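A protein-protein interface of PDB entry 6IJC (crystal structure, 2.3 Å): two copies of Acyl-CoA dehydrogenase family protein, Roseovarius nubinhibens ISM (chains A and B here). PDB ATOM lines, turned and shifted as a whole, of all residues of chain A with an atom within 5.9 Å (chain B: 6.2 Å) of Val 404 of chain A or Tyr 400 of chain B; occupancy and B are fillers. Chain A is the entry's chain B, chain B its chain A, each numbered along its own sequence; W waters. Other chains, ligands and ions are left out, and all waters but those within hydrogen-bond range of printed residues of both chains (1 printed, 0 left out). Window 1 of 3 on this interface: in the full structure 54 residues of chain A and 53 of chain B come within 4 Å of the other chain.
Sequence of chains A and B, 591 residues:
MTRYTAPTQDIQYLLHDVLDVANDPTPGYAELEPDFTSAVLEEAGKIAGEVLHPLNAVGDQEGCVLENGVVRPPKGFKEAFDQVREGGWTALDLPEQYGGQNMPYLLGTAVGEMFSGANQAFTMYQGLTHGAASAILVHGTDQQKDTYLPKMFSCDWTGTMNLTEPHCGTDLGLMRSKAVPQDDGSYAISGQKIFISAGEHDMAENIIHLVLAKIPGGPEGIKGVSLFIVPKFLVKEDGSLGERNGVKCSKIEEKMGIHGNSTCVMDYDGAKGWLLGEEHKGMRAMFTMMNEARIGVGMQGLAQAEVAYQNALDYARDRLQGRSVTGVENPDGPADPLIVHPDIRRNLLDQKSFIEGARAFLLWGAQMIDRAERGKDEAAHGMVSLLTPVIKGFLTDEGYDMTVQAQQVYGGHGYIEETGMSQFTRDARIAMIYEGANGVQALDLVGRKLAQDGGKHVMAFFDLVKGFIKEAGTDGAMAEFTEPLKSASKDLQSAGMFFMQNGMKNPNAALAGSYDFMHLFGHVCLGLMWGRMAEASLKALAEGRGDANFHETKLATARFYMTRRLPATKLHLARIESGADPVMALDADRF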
ATOM      1  N   GLY A 399      10.691 -23.451   3.576  1.00  0.00           N
ATOM      2  CA  GLY A 399       9.605 -22.568   3.188  1.00  0.00           C
ATOM      3  C   GLY A 399       9.641 -22.230   1.715  1.00  0.00           C
ATOM      4  O   GLY A 399       8.620 -22.282   1.034  1.00  0.00           O
ATOM      5  N   TYR A 400      10.818 -21.875   1.203  1.00  0.00           N
ATOM      6  CA  TYR A 400      10.968 -21.669  -0.236  1.00  0.00           C
ATOM      7  C   TYR A 400      10.575 -22.916  -1.029  1.00  0.00           C
ATOM      8  O   TYR A 400       9.831 -22.823  -2.014  1.00  0.00           O
ATOM      9  CB  TYR A 400      12.410 -21.283  -0.573  1.00  0.00           C
ATOM     10  CG  TYR A 400      12.637 -21.106  -2.063  1.00  0.00           C
ATOM     11  CD1 TYR A 400      12.279 -19.922  -2.688  1.00  0.00           C
ATOM     12  CD2 TYR A 400      13.203 -22.121  -2.839  1.00  0.00           C
ATOM     13  CE1 TYR A 400      12.470 -19.738  -4.053  1.00  0.00           C
ATOM     14  CE2 TYR A 400      13.395 -21.948  -4.211  1.00  0.00           C
ATOM     15  CZ  TYR A 400      13.022 -20.749  -4.802  1.00  0.00           C
ATOM     16  OH  TYR A 400      13.211 -20.531  -6.139  1.00  0.00           O
ATOM     17  N   ASP A 401      11.103 -24.089  -0.638  1.00  0.00           N
ATOM     18  CA  ASP A 401      10.781 -25.330  -1.347  1.00  0.00           C
ATOM     19  C   ASP A 401       9.281 -25.556  -1.389  1.00  0.00           C
ATOM     20  O   ASP A 401       8.738 -26.012  -2.399  1.00  0.00           O
ATOM     21  CB  ASP A 401      11.453 -26.527  -0.688  1.00  0.00           C
ATOM     22  CG  ASP A 401      12.920 -26.653  -1.052  1.00  0.00           C
ATOM     23  OD1 ASP A 401      13.302 -26.239  -2.171  1.00  0.00           O
ATOM     24  OD2 ASP A 401      13.695 -27.178  -0.213  1.00  0.00           O
ATOM     25  N   MET A 402       8.591 -25.225  -0.305  1.00  0.00           N
ATOM     26  CA  MET A 402       7.156 -25.422  -0.296  1.00  0.00           C
ATOM     27  C   MET A 402       6.467 -24.462  -1.249  1.00  0.00           C
ATOM     28  O   MET A 402       5.516 -24.859  -1.936  1.00  0.00           O
ATOM     29  CB  MET A 402       6.623 -25.292   1.130  1.00  0.00           C
ATOM     30  CG  MET A 402       7.191 -26.373   2.062  1.00  0.00           C
ATOM     31  SD  MET A 402       6.905 -28.082   1.518  1.00  0.00           S
ATOM     32  CE  MET A 402       8.513 -28.574   0.903  1.00  0.00           C
ATOM     33  N   THR A 403       6.934 -23.202  -1.328  1.00  0.00           N
ATOM     34  CA  THR A 403       6.321 -22.278  -2.284  1.00  0.00           C
ATOM     35  C   THR A 403       6.483 -22.793  -3.703  1.00  0.00           C
ATOM     36  O   THR A 403       5.559 -22.677  -4.516  1.00  0.00           O
ATOM     37  CB  THR A 403       6.886 -20.850  -2.178  1.00  0.00           C
ATOM     38  OG1 THR A 403       8.283 -20.838  -2.512  1.00  0.00           O
ATOM     39  CG2 THR A 403       6.677 -20.256  -0.785  1.00  0.00           C
ATOM     40  N   VAL A 404       7.641 -23.386  -4.013  1.00  0.00           N
ATOM     41  CA  VAL A 404       7.831 -24.015  -5.318  1.00  0.00           C
ATOM     42  C   VAL A 404       6.817 -25.141  -5.516  1.00  0.00           C
ATOM     43  O   VAL A 404       6.159 -25.231  -6.568  1.00  0.00           O
ATOM     44  CB  VAL A 404       9.280 -24.513  -5.474  1.00  0.00           C
ATOM     45  CG1 VAL A 404       9.449 -25.286  -6.784  1.00  0.00           C
ATOM     46  CG2 VAL A 404      10.264 -23.340  -5.402  1.00  0.00           C
ATOM     47  N   GLN A 405       6.655 -25.997  -4.495  1.00  0.00           N
ATOM     48  CA  GLN A 405       5.698 -27.100  -4.583  1.00  0.00           C
ATOM     49  C   GLN A 405       4.266 -26.594  -4.704  1.00  0.00           C
ATOM     50  O   GLN A 405       3.438 -27.221  -5.382  1.00  0.00           O
ATOM     51  CB  GLN A 405       5.825 -28.024  -3.362  1.00  0.00           C
ATOM     52  CG  GLN A 405       7.117 -28.858  -3.361  1.00  0.00           C
ATOM     53  CD  GLN A 405       7.153 -29.913  -2.261  1.00  0.00           C
ATOM     54  OE1 GLN A 405       6.109 -30.376  -1.779  1.00  0.00           O
ATOM     55  NE2 GLN A 405       8.357 -30.310  -1.873  1.00  0.00           N
ATOM     56  N   ALA A 406       3.935 -25.493  -4.016  1.00  0.00           N
ATOM     57  CA  ALA A 406       2.598 -24.921  -4.169  1.00  0.00           C
ATOM     58  C   ALA A 406       2.383 -24.418  -5.592  1.00  0.00           C
ATOM     59  O   ALA A 406       1.310 -24.624  -6.176  1.00  0.00           O
ATOM     60  CB  ALA A 406       2.369 -23.786  -3.160  1.00  0.00           C
ATOM     61  N   GLN A 407       3.389 -23.741  -6.160  1.00  0.00           N
ATOM     62  CA  GLN A 407       3.309 -23.306  -7.556  1.00  0.00           C
ATOM     63  C   GLN A 407       3.129 -24.491  -8.501  1.00  0.00           C
ATOM     64  O   GLN A 407       2.421 -24.386  -9.515  1.00  0.00           O
ATOM     65  CB  GLN A 407       4.566 -22.523  -7.922  1.00  0.00           C
ATOM     66  CG  GLN A 407       4.674 -22.085  -9.364  1.00  0.00           C
ATOM     67  CD  GLN A 407       6.040 -21.451  -9.657  1.00  0.00           C
ATOM     68  OE1 GLN A 407       7.048 -21.813  -9.038  1.00  0.00           O
ATOM     69  NE2 GLN A 407       6.076 -20.506 -10.590  1.00  0.00           N
ATOM     70  N   GLN A 408       3.757 -25.628  -8.176  1.00  0.00           N
ATOM     71  CA  GLN A 408       3.624 -26.829  -8.993  1.00  0.00           C
ATOM     72  C   GLN A 408       2.181 -27.335  -9.045  1.00  0.00           C
ATOM     73  O   GLN A 408       1.767 -27.908 -10.063  1.00  0.00           O
ATOM     74  CB  GLN A 408       4.560 -27.917  -8.459  1.00  0.00           C
ATOM     75  CG  GLN A 408       4.663 -29.153  -9.339  1.00  0.00           C
ATOM     76  CD  GLN A 408       5.504 -28.954 -10.598  1.00  0.00           C
ATOM     77  OE1 GLN A 408       6.243 -27.959 -10.745  1.00  0.00           O
ATOM     78  NE2 GLN A 408       5.407 -29.923 -11.516  1.00  0.00           N
ATOM     79  N   VAL A 409       1.407 -27.148  -7.963  1.00  0.00           N
ATOM     80  CA  VAL A 409       0.014 -27.600  -7.930  1.00  0.00           C
ATOM     81  C   VAL A 409      -0.806 -26.947  -9.049  1.00  0.00           C
ATOM     82  O   VAL A 409      -1.746 -27.553  -9.579  1.00  0.00           O
ATOM     83  CB  VAL A 409      -0.586 -27.328  -6.528  1.00  0.00           C
ATOM     84  CG1 VAL A 409      -2.131 -27.310  -6.537  1.00  0.00           C
ATOM     85  CG2 VAL A 409      -0.097 -28.380  -5.548  1.00  0.00           C
ATOM     86  N   THR A 425       7.272 -17.623  -4.576  1.00  0.00           N
ATOM     87  CA  THR A 425       8.629 -18.181  -4.556  1.00  0.00           C
ATOM     88  C   THR A 425       9.681 -17.072  -4.621  1.00  0.00           C
ATOM     89  O   THR A 425      10.650 -17.078  -3.850  1.00  0.00           O
ATOM     90  CB  THR A 425       8.869 -19.196  -5.698  1.00  0.00           C
ATOM     91  OG1 THR A 425       9.263 -18.515  -6.909  1.00  0.00           O
ATOM     92  CG2 THR A 425       7.637 -20.083  -5.943  1.00  0.00           C
ATOM     93  N   MET B 256       7.007 -16.439 -15.861  1.00  0.00           N
ATOM     94  CA  MET B 256       8.056 -16.303 -14.854  1.00  0.00           C
ATOM     95  C   MET B 256       9.438 -16.223 -15.488  1.00  0.00           C
ATOM     96  O   MET B 256      10.318 -15.514 -14.976  1.00  0.00           O
ATOM     97  CB  MET B 256       7.968 -17.478 -13.881  1.00  0.00           C
ATOM     98  CG  MET B 256       8.966 -17.462 -12.751  1.00  0.00           C
ATOM     99  SD  MET B 256       8.821 -18.961 -11.766  1.00  0.00           S
ATOM    100  CE  MET B 256       9.781 -18.521 -10.301  1.00  0.00           C
ATOM    101  N   GLY B 301      16.499 -29.235 -18.346  1.00  0.00           N
ATOM    102  CA  GLY B 301      16.803 -29.085 -16.932  1.00  0.00           C
ATOM    103  C   GLY B 301      18.283 -29.238 -16.635  1.00  0.00           C
ATOM    104  O   GLY B 301      18.859 -28.459 -15.876  1.00  0.00           O
ATOM    105  N   ALA B 305      21.172 -26.206 -15.235  1.00  0.00           N
ATOM    106  CA  ALA B 305      22.102 -26.414 -14.128  1.00  0.00           C
ATOM    107  C   ALA B 305      23.547 -26.258 -14.585  1.00  0.00           C
ATOM    108  O   ALA B 305      24.390 -25.770 -13.829  1.00  0.00           O
ATOM    109  CB  ALA B 305      21.903 -27.795 -13.501  1.00  0.00           C
ATOM    110  N   PHE B 354      25.788 -33.907  -9.626  1.00  0.00           N
ATOM    111  CA  PHE B 354      24.517 -34.109 -10.320  1.00  0.00           C
ATOM    112  C   PHE B 354      24.667 -33.910 -11.823  1.00  0.00           C
ATOM    113  O   PHE B 354      24.242 -34.764 -12.610  1.00  0.00           O
ATOM    114  CB  PHE B 354      23.426 -33.172  -9.823  1.00  0.00           C
ATOM    115  CG  PHE B 354      22.276 -33.069 -10.798  1.00  0.00           C
ATOM    116  CD1 PHE B 354      21.392 -34.127 -10.950  1.00  0.00           C
ATOM    117  CD2 PHE B 354      22.117 -31.944 -11.593  1.00  0.00           C
ATOM    118  CE1 PHE B 354      20.354 -34.059 -11.870  1.00  0.00           C
ATOM    119  CE2 PHE B 354      21.091 -31.865 -12.496  1.00  0.00           C
ATOM    120  CZ  PHE B 354      20.197 -32.919 -12.635  1.00  0.00           C
ATOM    121  N   LEU B 395      15.656 -35.085 -13.766  1.00  0.00           N
ATOM    122  CA  LEU B 395      16.662 -34.133 -14.212  1.00  0.00           C
ATOM    123  C   LEU B 395      16.152 -32.708 -14.119  1.00  0.00           C
ATOM    124  O   LEU B 395      16.941 -31.793 -13.851  1.00  0.00           O
ATOM    125  CB  LEU B 395      17.111 -34.443 -15.638  1.00  0.00           C
ATOM    126  CG  LEU B 395      18.418 -35.235 -15.768  1.00  0.00           C
ATOM    127  CD1 LEU B 395      18.382 -36.571 -15.028  1.00  0.00           C
ATOM    128  CD2 LEU B 395      18.751 -35.452 -17.246  1.00  0.00           C
ATOM    129  N   THR B 396      14.842 -32.498 -14.317  1.00  0.00           N
ATOM    130  CA  THR B 396      14.300 -31.148 -14.191  1.00  0.00           C
ATOM    131  C   THR B 396      14.123 -30.727 -12.733  1.00  0.00           C
ATOM    132  O   THR B 396      14.301 -29.543 -12.417  1.00  0.00           O
ATOM    133  CB  THR B 396      12.970 -31.019 -14.947  1.00  0.00           C
ATOM    134  OG1 THR B 396      12.047 -32.020 -14.500  1.00  0.00           O
ATOM    135  CG2 THR B 396      13.190 -31.167 -16.413  1.00  0.00           C
ATOM    136  N   ASP B 397      13.778 -31.655 -11.834  1.00  0.00           N
ATOM    137  CA  ASP B 397      13.680 -31.306 -10.417  1.00  0.00           C
ATOM    138  C   ASP B 397      15.054 -30.995  -9.854  1.00  0.00           C
ATOM    139  O   ASP B 397      15.270 -29.924  -9.278  1.00  0.00           O
ATOM    140  CB  ASP B 397      13.045 -32.434  -9.590  1.00  0.00           C
ATOM    141  CG  ASP B 397      11.541 -32.451  -9.675  1.00  0.00           C
ATOM    142  OD1 ASP B 397      10.951 -31.435 -10.113  1.00  0.00           O
ATOM    143  OD2 ASP B 397      10.953 -33.490  -9.297  1.00  0.00           O
ATOM    144  N   GLU B 398      15.988 -31.946  -9.983  1.00  0.00           N
ATOM    145  CA  GLU B 398      17.342 -31.725  -9.484  1.00  0.00           C
ATOM    146  C   GLU B 398      17.992 -30.563 -10.214  1.00  0.00           C
ATOM    147  O   GLU B 398      18.699 -29.755  -9.604  1.00  0.00           O
ATOM    148  CB  GLU B 398      18.189 -32.989  -9.641  1.00  0.00           C
ATOM    149  CG  GLU B 398      17.743 -34.206  -8.820  1.00  0.00           C
ATOM    150  CD  GLU B 398      18.068 -34.074  -7.332  1.00  0.00           C
ATOM    151  OE1 GLU B 398      17.271 -33.463  -6.593  1.00  0.00           O
ATOM    152  OE2 GLU B 398      19.120 -34.576  -6.898  1.00  0.00           O
ATOM    153  N   GLY B 399      17.727 -30.444 -11.519  1.00  0.00           N
ATOM    154  CA  GLY B 399      18.308 -29.358 -12.288  1.00  0.00           C
ATOM    155  C   GLY B 399      17.897 -28.002 -11.756  1.00  0.00           C
ATOM    156  O   GLY B 399      18.725 -27.104 -11.596  1.00  0.00           O
ATOM    157  N   TYR B 400      16.609 -27.839 -11.465  1.00  0.00           N
ATOM    158  CA  TYR B 400      16.142 -26.581 -10.885  1.00  0.00           C
ATOM    159  C   TYR B 400      16.801 -26.315  -9.533  1.00  0.00           C
ATOM    160  O   TYR B 400      17.289 -25.206  -9.277  1.00  0.00           O
ATOM    161  CB  TYR B 400      14.620 -26.591 -10.744  1.00  0.00           C
ATOM    162  CG  TYR B 400      14.075 -25.347 -10.049  1.00  0.00           C
ATOM    163  CD1 TYR B 400      13.944 -24.150 -10.743  1.00  0.00           C
ATOM    164  CD2 TYR B 400      13.707 -25.378  -8.700  1.00  0.00           C
ATOM    165  CE1 TYR B 400      13.471 -23.028 -10.131  1.00  0.00           C
ATOM    166  CE2 TYR B 400      13.228 -24.259  -8.075  1.00  0.00           C
ATOM    167  CZ  TYR B 400      13.109 -23.077  -8.805  1.00  0.00           C
ATOM    168  OH  TYR B 400      12.635 -21.945  -8.213  1.00  0.00           O
ATOM    169  N   ASP B 401      16.830 -27.327  -8.654  1.00  0.00           N
ATOM    170  CA  ASP B 401      17.455 -27.151  -7.340  1.00  0.00           C
ATOM    171  C   ASP B 401      18.909 -26.713  -7.465  1.00  0.00           C
ATOM    172  O   ASP B 401      19.370 -25.852  -6.706  1.00  0.00           O
ATOM    173  CB  ASP B 401      17.362 -28.440  -6.520  1.00  0.00           C
ATOM    174  CG  ASP B 401      15.948 -28.730  -6.022  1.00  0.00           C
ATOM    175  OD1 ASP B 401      15.098 -27.796  -5.993  1.00  0.00           O
ATOM    176  OD2 ASP B 401      15.684 -29.903  -5.654  1.00  0.00           O
ATOM    177  N   MET B 402      19.654 -27.299  -8.411  1.00  0.00           N
ATOM    178  CA  MET B 402      21.038 -26.883  -8.585  1.00  0.00           C
ATOM    179  C   MET B 402      21.140 -25.421  -9.027  1.00  0.00           C
ATOM    180  O   MET B 402      22.034 -24.704  -8.567  1.00  0.00           O
ATOM    181  CB  MET B 402      21.761 -27.812  -9.559  1.00  0.00           C
ATOM    182  CG  MET B 402      21.960 -29.241  -9.014  1.00  0.00           C
ATOM    183  SD  MET B 402      22.567 -29.385  -7.291  1.00  0.00           S
ATOM    184  CE  MET B 402      21.068 -29.754  -6.390  1.00  0.00           C
ATOM    185  N   THR B 403      20.236 -24.951  -9.910  1.00  0.00           N
ATOM    186  CA  THR B 403      20.325 -23.547 -10.318  1.00  0.00           C
ATOM    187  C   THR B 403      20.015 -22.613  -9.150  1.00  0.00           C
ATOM    188  O   THR B 403      20.537 -21.497  -9.108  1.00  0.00           O
ATOM    189  CB  THR B 403      19.401 -23.206 -11.512  1.00  0.00           C
ATOM    190  OG1 THR B 403      18.017 -23.245 -11.132  1.00  0.00           O
ATOM    191  CG2 THR B 403      19.632 -24.117 -12.705  1.00  0.00           C
ATOM    192  N   VAL B 404      19.182 -23.048  -8.197  1.00  0.00           N
ATOM    193  CA  VAL B 404      18.924 -22.239  -7.009  1.00  0.00           C
ATOM    194  C   VAL B 404      20.161 -22.191  -6.116  1.00  0.00           C
ATOM    195  O   VAL B 404      20.484 -21.147  -5.530  1.00  0.00           O
ATOM    196  CB  VAL B 404      17.691 -22.785  -6.261  1.00  0.00           C
ATOM    197  CG1 VAL B 404      17.579 -22.186  -4.860  1.00  0.00           C
ATOM    198  CG2 VAL B 404      16.414 -22.529  -7.061  1.00  0.00           C
ATOM    199  N   GLN B 405      20.873 -23.319  -6.010  1.00  0.00           N
ATOM    200  CA  GLN B 405      22.116 -23.384  -5.242  1.00  0.00           C
ATOM    201  C   GLN B 405      23.222 -22.590  -5.924  1.00  0.00           C
ATOM    202  O   GLN B 405      24.038 -21.941  -5.253  1.00  0.00           O
ATOM    203  CB  GLN B 405      22.551 -24.848  -5.068  1.00  0.00           C
ATOM    204  CG  GLN B 405      21.606 -25.701  -4.219  1.00  0.00           C
ATOM    205  CD  GLN B 405      22.131 -27.119  -3.998  1.00  0.00           C
ATOM    206  OE1 GLN B 405      23.331 -27.413  -4.207  1.00  0.00           O
ATOM    207  NE2 GLN B 405      21.244 -28.008  -3.544  1.00  0.00           N
ATOM    208  N   PHE B 424      18.442 -17.991 -14.691  1.00  0.00           N
ATOM    209  CA  PHE B 424      18.716 -19.415 -14.835  1.00  0.00           C
ATOM    210  C   PHE B 424      17.684 -20.247 -14.090  1.00  0.00           C
ATOM    211  O   PHE B 424      17.209 -21.258 -14.612  1.00  0.00           O
ATOM    212  CB  PHE B 424      20.133 -19.732 -14.356  1.00  0.00           C
ATOM    213  CG  PHE B 424      21.215 -19.120 -15.216  1.00  0.00           C
ATOM    214  CD1 PHE B 424      21.013 -18.913 -16.581  1.00  0.00           C
ATOM    215  CD2 PHE B 424      22.444 -18.764 -14.666  1.00  0.00           C
ATOM    216  CE1 PHE B 424      22.020 -18.359 -17.378  1.00  0.00           C
ATOM    217  CE2 PHE B 424      23.445 -18.211 -15.459  1.00  0.00           C
ATOM    218  CZ  PHE B 424      23.234 -17.992 -16.806  1.00  0.00           C
ATOM    219  N   THR B 425      17.285 -19.814 -12.884  1.00  0.00           N
ATOM    220  CA  THR B 425      16.296 -20.583 -12.130  1.00  0.00           C
ATOM    221  C   THR B 425      14.901 -20.422 -12.721  1.00  0.00           C
ATOM    222  O   THR B 425      14.139 -21.396 -12.821  1.00  0.00           O
ATOM    223  CB  THR B 425      16.285 -20.161 -10.661  1.00  0.00           C
ATOM    224  OG1 THR B 425      15.493 -18.976 -10.510  1.00  0.00           O
ATOM    225  CG2 THR B 425      17.704 -19.897 -10.148  1.00  0.00           C
ATOM    226  N   ARG B 426      14.543 -19.195 -13.106  1.00  0.00           N
ATOM    227  CA  ARG B 426      13.205 -18.955 -13.632  1.00  0.00           C
ATOM    228  C   ARG B 426      13.003 -19.697 -14.945  1.00  0.00           C
ATOM    229  O   ARG B 426      11.919 -20.228 -15.205  1.00  0.00           O
ATOM    230  CB  ARG B 426      12.972 -17.447 -13.801  1.00  0.00           C
ATOM    231  CG  ARG B 426      12.857 -16.696 -12.477  1.00  0.00           C
ATOM    232  CD  ARG B 426      12.589 -15.219 -12.676  1.00  0.00           C
ATOM    233  NE  ARG B 426      13.770 -14.480 -13.092  1.00  0.00           N
ATOM    234  CZ  ARG B 426      13.980 -14.015 -14.329  1.00  0.00           C
ATOM    235  NH1 ARG B 426      13.069 -14.218 -15.272  1.00  0.00           N
ATOM    236  NH2 ARG B 426      15.091 -13.325 -14.615  1.00  0.00           N
ATOM    237  N   ALA B 428      14.620 -22.487 -15.828  1.00  0.00           N
ATOM    238  CA  ALA B 428      14.574 -23.905 -15.478  1.00  0.00           C
ATOM    239  C   ALA B 428      13.224 -24.316 -14.915  1.00  0.00           C
ATOM    240  O   ALA B 428      12.856 -25.494 -14.994  1.00  0.00           O
ATOM    241  CB  ALA B 428      15.661 -24.230 -14.456  1.00  0.00           C
ATOM    242  N   ARG B 429      12.486 -23.375 -14.320  1.00  0.00           N
ATOM    243  CA  ARG B 429      11.283 -23.746 -13.585  1.00  0.00           C
ATOM    244  C   ARG B 429      10.246 -24.394 -14.503  1.00  0.00           C
ATOM    245  O   ARG B 429       9.535 -25.312 -14.086  1.00  0.00           O
ATOM    246  CB  ARG B 429      10.704 -22.516 -12.855  1.00  0.00           C
ATOM    247  CG  ARG B 429       9.419 -22.767 -12.027  1.00  0.00           C
ATOM    248  CD  ARG B 429       9.687 -23.496 -10.699  1.00  0.00           C
ATOM    249  NE  ARG B 429       8.465 -23.914  -9.995  1.00  0.00           N
ATOM    250  CZ  ARG B 429       7.776 -25.028 -10.254  1.00  0.00           C
ATOM    251  NH1 ARG B 429       8.165 -25.869 -11.214  1.00  0.00           N
ATOM    252  NH2 ARG B 429       6.691 -25.304  -9.554  1.00  0.00           N
ATOM    253  N   MET B 432       9.958 -28.444 -15.300  1.00  0.00           N
ATOM    254  CA  MET B 432       9.248 -29.312 -14.370  1.00  0.00           C
ATOM    255  C   MET B 432       7.749 -29.326 -14.609  1.00  0.00           C
ATOM    256  O   MET B 432       7.067 -30.212 -14.079  1.00  0.00           O
ATOM    257  CB  MET B 432       9.502 -28.871 -12.919  1.00  0.00           C
ATOM    258  CG  MET B 432      10.978 -28.752 -12.532  1.00  0.00           C
ATOM    259  SD  MET B 432      11.185 -27.936 -10.932  1.00  0.00           S
ATOM    260  CE  MET B 432      11.265 -26.288 -11.431  1.00  0.00           C
HETATM  261  O   HOH W   1      12.715 -26.159  -4.867  1.00  0.00           O
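Tyr 400 of chain B touches its own counterpart, Tyr 400 of chain A. Tyr 400 of chain A touches Val 404 of chain B, and with the chains exchanged Val 404 of chain A touches Tyr 400 of chain B. Positions printed for both chains: 399, 400, 401, 402, 403, 404, 405 and 425. Of the 9 pairs that touch across the chains among the printed residues, 3 have their exchanged pair printed and touching as well.
Water W1 lies within hydrogen-bond range of OD1 of Asp 401 of chain A (2.8 Å) and OD1 of Asp 401 of chain B (3.1 Å).
NH1 of Arg 426 of chain B is in hydrogen-bond range of O of Met 256 of chain B (3.1 Å). OG1 of Thr 403 of chain B is in hydrogen-bond range of O of Tyr 400 of chain B, 2.8 Å away. The guanidinium group of Arg 429 of chain B sits close to the side-chain sulfur of Met 432 of chain B (3.7 Å). The backbone carbonyl oxygen of Tyr 400 of chain A lies within hydrogen-bond range of the side-chain hydroxyl of Thr 403 of chain A (2.6 Å).
OH of Tyr 400 of chain A touches CG2 of Val 404 of chain B, at 3.9 Å. CG2 of Val 404 of chain A touches OH of Tyr 400 of chain B, 3.9 Å away. CE of Met 256 of chain B touches OG1 of Thr 425 of chain A, at 3.4 Å.
The side-chain sulfur (SD) of Met 256 of chain B lies within hydrogen-bond range of the side-chain amide nitrogen (NE2) of Gln 407 of chain A (3.4 Å). OH of Tyr 400 of chain B sits at hydrogen-bond distance from OH of Tyr 400 of chain A, at 2.6 Å. The guanidinium group (NH2) of Arg 429 of chain B sits at hydrogen-bond distance from the backbone carbonyl oxygen (O) of Val 404 of chain A. OE1 of Gln 407 of chain A lies within hydrogen-bond range of NE of Arg 429 of chain B (2.7 Å). NH1 of Arg 429 of chain B is in hydrogen-bond range of OE1 of Gln 408 of chain A, 2.9 Å away. The side-chain amide nitrogen (NE2) of Gln 408 of chain A is in hydrogen-bond range of the backbone carbonyl oxygen (O) of Met 432 of chain B, 3.1 Å away.
Printed residues of chain B within 4 Å of Val 404 of chain A: Tyr 400 and Arg 429. Of the printed residues of chain B, Gln 407 of chain A touches Met 256 and Arg 429. Printed residues of chain B within 4 Å of Gln 408 of chain A: Arg 429 (2.9 Å) and Met 432 (3.1 Å). Of the printed residues of chain B, Thr 425 of chain A touches Met 256. Of the printed residues of chain A, Tyr 400 of chain B touches Tyr 400 and Val 404. Printed residues of chain A within 4 Å of Val 404 of chain B: Tyr 400 (3.9 Å). Of the printed residues of chain A, Met 432 of chain B touches Gln 408. The nearest residue of chain B that does not touch Val 404 of chain A is Met 432 of chain B (5.1 Å). The nearest residue of chain A that does not touch Tyr 400 of chain B is Thr 425 of chain A (5.0 Å). The nearest printed residue of chain A that does not touch Met 432 of chain B is Val 404 of chain A (5.1 Å).
Hydrophobic or aromatic side chains of chain B within 4 Å of the printed part of chain A: Met 256, Tyr 400 and Val 404. Among the printed residues, no Asp or Glu carboxylate lies within 4 Å of a Lys or Arg side-chain nitrogen of the other chain.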
